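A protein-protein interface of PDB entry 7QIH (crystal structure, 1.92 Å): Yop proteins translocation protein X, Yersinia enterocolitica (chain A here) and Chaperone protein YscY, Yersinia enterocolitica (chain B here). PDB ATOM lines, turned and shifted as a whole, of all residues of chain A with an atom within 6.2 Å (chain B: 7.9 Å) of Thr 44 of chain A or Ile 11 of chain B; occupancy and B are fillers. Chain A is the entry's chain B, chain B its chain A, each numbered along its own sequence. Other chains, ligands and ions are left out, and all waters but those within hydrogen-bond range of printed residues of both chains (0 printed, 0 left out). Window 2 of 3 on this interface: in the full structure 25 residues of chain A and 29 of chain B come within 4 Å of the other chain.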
ATOM      1  N   GLN A  39      30.476 -24.409  26.624  1.00  0.00           N
ATOM      2  CA  GLN A  39      31.139 -23.121  26.432  1.00  0.00           C
ATOM      3  C   GLN A  39      32.127 -23.175  25.273  1.00  0.00           C
ATOM      4  O   GLN A  39      32.253 -22.206  24.515  1.00  0.00           O
ATOM      5  CB  GLN A  39      31.827 -22.671  27.725  1.00  0.00           C
ATOM      6  CG  GLN A  39      32.819 -23.657  28.323  1.00  0.00           C
ATOM      7  CD  GLN A  39      34.225 -23.485  27.786  1.00  0.00           C
ATOM      8  OE1 GLN A  39      34.499 -22.561  27.022  1.00  0.00           O
ATOM      9  NE2 GLN A  39      35.126 -24.377  28.183  1.00  0.00           N
ATOM     10  N   SER A  40      32.829 -24.299  25.110  1.00  0.00           N
ATOM     11  CA  SER A  40      33.724 -24.437  23.966  1.00  0.00           C
ATOM     12  C   SER A  40      32.947 -24.643  22.673  1.00  0.00           C
ATOM     13  O   SER A  40      33.389 -24.195  21.609  1.00  0.00           O
ATOM     14  CB  SER A  40      34.699 -25.593  24.191  1.00  0.00           C
ATOM     15  OG  SER A  40      34.010 -26.826  24.287  1.00  0.00           O
ATOM     16  N   LEU A  41      31.793 -25.310  22.745  1.00  0.00           N
ATOM     17  CA  LEU A  41      30.961 -25.493  21.559  1.00  0.00           C
ATOM     18  C   LEU A  41      30.417 -24.160  21.057  1.00  0.00           C
ATOM     19  O   LEU A  41      30.560 -23.822  19.876  1.00  0.00           O
ATOM     20  CB  LEU A  41      29.817 -26.459  21.870  1.00  0.00           C
ATOM     21  CG  LEU A  41      28.836 -26.751  20.733  1.00  0.00           C
ATOM     22  CD1 LEU A  41      29.550 -27.409  19.563  1.00  0.00           C
ATOM     23  CD2 LEU A  41      27.688 -27.621  21.222  1.00  0.00           C
ATOM     24  N   LEU A  42      29.789 -23.383  21.945  1.00  0.00           N
ATOM     25  CA  LEU A  42      29.191 -22.117  21.539  1.00  0.00           C
ATOM     26  C   LEU A  42      30.233 -21.067  21.163  1.00  0.00           C
ATOM     27  O   LEU A  42      29.893 -20.097  20.475  1.00  0.00           O
ATOM     28  CB  LEU A  42      28.290 -21.577  22.654  1.00  0.00           C
ATOM     29  CG  LEU A  42      27.112 -22.442  23.117  1.00  0.00           C
ATOM     30  CD1 LEU A  42      26.280 -21.698  24.152  1.00  0.00           C
ATOM     31  CD2 LEU A  42      26.245 -22.878  21.947  1.00  0.00           C
ATOM     32  N   THR A  43      31.486 -21.227  21.599  1.00  0.00           N
ATOM     33  CA  THR A  43      32.523 -20.267  21.233  1.00  0.00           C
ATOM     34  C   THR A  43      32.820 -20.305  19.737  1.00  0.00           C
ATOM     35  O   THR A  43      33.128 -19.267  19.140  1.00  0.00           O
ATOM     36  CB  THR A  43      33.800 -20.535  22.035  1.00  0.00           C
ATOM     37  OG1 THR A  43      33.516 -20.445  23.435  1.00  0.00           O
ATOM     38  CG2 THR A  43      34.879 -19.522  21.689  1.00  0.00           C
ATOM     39  N   THR A  44      32.716 -21.481  19.115  1.00  0.00           N
ATOM     40  CA  THR A  44      32.989 -21.619  17.690  1.00  0.00           C
ATOM     41  C   THR A  44      31.933 -20.957  16.814  1.00  0.00           C
ATOM     42  O   THR A  44      32.118 -20.893  15.594  1.00  0.00           O
ATOM     43  CB  THR A  44      33.096 -23.100  17.318  1.00  0.00           C
ATOM     44  OG1 THR A  44      31.795 -23.699  17.362  1.00  0.00           O
ATOM     45  CG2 THR A  44      34.006 -23.831  18.292  1.00  0.00           C
ATOM     46  N   SER A  45      30.846 -20.463  17.397  1.00  0.00           N
ATOM     47  CA  SER A  45      29.766 -19.886  16.614  1.00  0.00           C
ATOM     48  C   SER A  45      30.112 -18.471  16.163  1.00  0.00           C
ATOM     49  O   SER A  45      30.999 -17.810  16.709  1.00  0.00           O
ATOM     50  CB  SER A  45      28.466 -19.869  17.415  1.00  0.00           C
ATOM     51  OG  SER A  45      27.457 -19.157  16.719  1.00  0.00           O
ATOM     52  N   GLN A  46      29.384 -18.010  15.148  1.00  0.00           N
ATOM     53  CA  GLN A  46      29.524 -16.666  14.607  1.00  0.00           C
ATOM     54  C   GLN A  46      28.430 -15.722  15.086  1.00  0.00           C
ATOM     55  O   GLN A  46      28.570 -14.505  14.926  1.00  0.00           O
ATOM     56  CB  GLN A  46      29.522 -16.707  13.072  1.00  0.00           C
ATOM     57  CG  GLN A  46      28.232 -17.244  12.454  1.00  0.00           C
ATOM     58  CD  GLN A  46      28.079 -18.749  12.611  1.00  0.00           C
ATOM     59  OE1 GLN A  46      29.043 -19.501  12.462  1.00  0.00           O
ATOM     60  NE2 GLN A  46      26.866 -19.194  12.924  1.00  0.00           N
ATOM     61  N   LEU A  50      25.015 -16.366  20.639  1.00  0.00           N
ATOM     62  CA  LEU A  50      25.674 -17.579  21.110  1.00  0.00           C
ATOM     63  C   LEU A  50      27.043 -17.272  21.707  1.00  0.00           C
ATOM     64  O   LEU A  50      27.462 -17.930  22.666  1.00  0.00           O
ATOM     65  CB  LEU A  50      25.802 -18.589  19.970  1.00  0.00           C
ATOM     66  CG  LEU A  50      24.508 -19.091  19.323  1.00  0.00           C
ATOM     67  CD1 LEU A  50      24.799 -20.157  18.278  1.00  0.00           C
ATOM     68  CD2 LEU A  50      23.560 -19.628  20.376  1.00  0.00           C
ATOM     69  N   ASN B  10      27.913 -25.911  11.602  1.00  0.00           N
ATOM     70  CA  ASN B  10      26.572 -25.855  12.170  1.00  0.00           C
ATOM     71  C   ASN B  10      26.544 -26.545  13.533  1.00  0.00           C
ATOM     72  O   ASN B  10      27.085 -27.639  13.694  1.00  0.00           O
ATOM     73  CB  ASN B  10      25.561 -26.501  11.220  1.00  0.00           C
ATOM     74  CG  ASN B  10      24.185 -25.874  11.322  1.00  0.00           C
ATOM     75  OD1 ASN B  10      24.041 -24.737  11.770  1.00  0.00           O
ATOM     76  ND2 ASN B  10      23.165 -26.612  10.900  1.00  0.00           N
ATOM     77  N   ILE B  11      25.912 -25.902  14.511  1.00  0.00           N
ATOM     78  CA  ILE B  11      25.883 -26.385  15.888  1.00  0.00           C
ATOM     79  C   ILE B  11      24.544 -27.059  16.151  1.00  0.00           C
ATOM     80  O   ILE B  11      23.488 -26.523  15.791  1.00  0.00           O
ATOM     81  CB  ILE B  11      26.124 -25.239  16.885  1.00  0.00           C
ATOM     82  CG1 ILE B  11      27.522 -24.651  16.699  1.00  0.00           C
ATOM     83  CG2 ILE B  11      25.936 -25.719  18.317  1.00  0.00           C
ATOM     84  CD1 ILE B  11      27.831 -23.515  17.646  1.00  0.00           C
ATOM     85  N   THR B  12      24.587 -28.232  16.780  1.00  0.00           N
ATOM     86  CA  THR B  12      23.395 -28.942  17.222  1.00  0.00           C
ATOM     87  C   THR B  12      23.560 -29.296  18.692  1.00  0.00           C
ATOM     88  O   THR B  12      24.608 -29.814  19.095  1.00  0.00           O
ATOM     89  CB  THR B  12      23.154 -30.211  16.393  1.00  0.00           C
ATOM     90  OG1 THR B  12      23.055 -29.867  15.004  1.00  0.00           O
ATOM     91  CG2 THR B  12      21.871 -30.902  16.831  1.00  0.00           C
ATOM     92  N   LEU B  13      22.534 -29.012  19.492  1.00  0.00           N
ATOM     93  CA  LEU B  13      22.578 -29.260  20.926  1.00  0.00           C
ATOM     94  C   LEU B  13      22.037 -30.648  21.243  1.00  0.00           C
ATOM     95  O   LEU B  13      20.960 -31.025  20.771  1.00  0.00           O
ATOM     96  CB  LEU B  13      21.767 -28.208  21.683  1.00  0.00           C
ATOM     97  CG  LEU B  13      22.228 -26.753  21.625  1.00  0.00           C
ATOM     98  CD1 LEU B  13      21.300 -25.878  22.449  1.00  0.00           C
ATOM     99  CD2 LEU B  13      23.666 -26.622  22.109  1.00  0.00           C
ATOM    100  N   THR B  14      22.782 -31.402  22.047  1.00  0.00           N
ATOM    101  CA  THR B  14      22.250 -32.636  22.600  1.00  0.00           C
ATOM    102  C   THR B  14      21.117 -32.320  23.573  1.00  0.00           C
ATOM    103  O   THR B  14      20.919 -31.174  23.986  1.00  0.00           O
ATOM    104  CB  THR B  14      23.345 -33.429  23.314  1.00  0.00           C
ATOM    105  OG1 THR B  14      23.814 -32.679  24.442  1.00  0.00           O
ATOM    106  CG2 THR B  14      24.510 -33.706  22.379  1.00  0.00           C
ATOM    107  N   GLN B  17      22.496 -30.802  26.660  1.00  0.00           N
ATOM    108  CA  GLN B  17      22.888 -29.407  26.481  1.00  0.00           C
ATOM    109  C   GLN B  17      21.670 -28.495  26.415  1.00  0.00           C
ATOM    110  O   GLN B  17      21.689 -27.386  26.963  1.00  0.00           O
ATOM    111  CB  GLN B  17      23.750 -29.262  25.227  1.00  0.00           C
ATOM    112  CG  GLN B  17      25.131 -29.887  25.366  1.00  0.00           C
ATOM    113  CD  GLN B  17      25.869 -30.005  24.047  1.00  0.00           C
ATOM    114  OE1 GLN B  17      25.257 -30.051  22.981  1.00  0.00           O
ATOM    115  NE2 GLN B  17      27.194 -30.058  24.115  1.00  0.00           N
ATOM    116  N   THR B  46      17.697 -20.045  19.820  1.00  0.00           N
ATOM    117  CA  THR B  46      18.314 -19.851  18.514  1.00  0.00           C
ATOM    118  C   THR B  46      18.629 -21.189  17.858  1.00  0.00           C
ATOM    119  O   THR B  46      18.423 -21.364  16.651  1.00  0.00           O
ATOM    120  CB  THR B  46      19.585 -19.012  18.654  1.00  0.00           C
ATOM    121  OG1 THR B  46      19.248 -17.707  19.138  1.00  0.00           O
ATOM    122  CG2 THR B  46      20.305 -18.884  17.318  1.00  0.00           C
ATOM    123  N   LEU B  47      19.116 -22.150  18.642  1.00  0.00           N
ATOM    124  CA  LEU B  47      19.493 -23.454  18.114  1.00  0.00           C
ATOM    125  C   LEU B  47      18.340 -24.444  18.109  1.00  0.00           C
ATOM    126  O   LEU B  47      18.314 -25.347  17.265  1.00  0.00           O
ATOM    127  CB  LEU B  47      20.660 -24.025  18.924  1.00  0.00           C
ATOM    128  CG  LEU B  47      21.936 -23.186  18.830  1.00  0.00           C
ATOM    129  CD1 LEU B  47      23.054 -23.769  19.681  1.00  0.00           C
ATOM    130  CD2 LEU B  47      22.373 -23.066  17.380  1.00  0.00           C
ATOM    131  N   ASN B  48      17.386 -24.296  19.026  1.00  0.00           N
ATOM    132  CA  ASN B  48      16.213 -25.165  19.106  1.00  0.00           C
ATOM    133  C   ASN B  48      14.974 -24.286  19.207  1.00  0.00           C
ATOM    134  O   ASN B  48      14.417 -24.093  20.297  1.00  0.00           O
ATOM    135  CB  ASN B  48      16.329 -26.134  20.284  1.00  0.00           C
ATOM    136  CG  ASN B  48      17.436 -27.150  20.084  1.00  0.00           C
ATOM    137  OD1 ASN B  48      18.620 -26.839  20.246  1.00  0.00           O
ATOM    138  ND2 ASN B  48      17.059 -28.369  19.715  1.00  0.00           N
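Among the printed residues, merely in contact across the chains: Leu 41 of chain A with Ile 11 of chain B (3.5 Å), Ser 45 of chain A with Ile 11 of chain B (3.7 Å), Leu 41 of chain A with Gln 17 of chain B (3.8 Å), Leu 50 of chain A with Leu 47 of chain B (3.9 Å) and Thr 44 of chain A with Ile 11 of chain B (3.98 Å).
The backbone NH of Thr 14 of chain B is in hydrogen-bond range of the side-chain amide oxygen of Gln 17 of chain B.
The side-chain hydroxyl (OG1) of Thr 44 of chain A lies within hydrogen-bond range of the backbone carbonyl oxygen (O) of Leu 41 of chain A, at 2.8 Å.
Of the printed residues of chain B, Leu 41 of chain A touches Ile 11 and Gln 17.
Printed residues of chain B within 4 Å of Thr 44 of chain A: Ile 11 (3.98 Å).
Of the printed residues of chain B, Leu 50 of chain A touches Leu 47.
Printed residues of chain A within 4 Å of Ile 11 of chain B: Leu 41, Thr 44 and Ser 45.
Of the printed residues of chain A, Gln 17 of chain B touches Leu 41 (3.8 Å).
Of the printed residues of chain A, Leu 47 of chain B touches Leu 50.
The nearest residue of chain B that does not touch Thr 44 of chain A is Asn 10 of chain B (7.1 Å).
Printed residues of chain B that touch a printed residue of chain A: Ile 11, Gln 17 and Leu 47.
Of the 9 printed residues of chain A, 4 touch a printed residue of chain B.
Hydrophobic or aromatic side chains of chain A within 4 Å of the printed part of chain B: Leu 41 and Leu 50.
Among the printed residues, 5 pairs touch across the chains.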
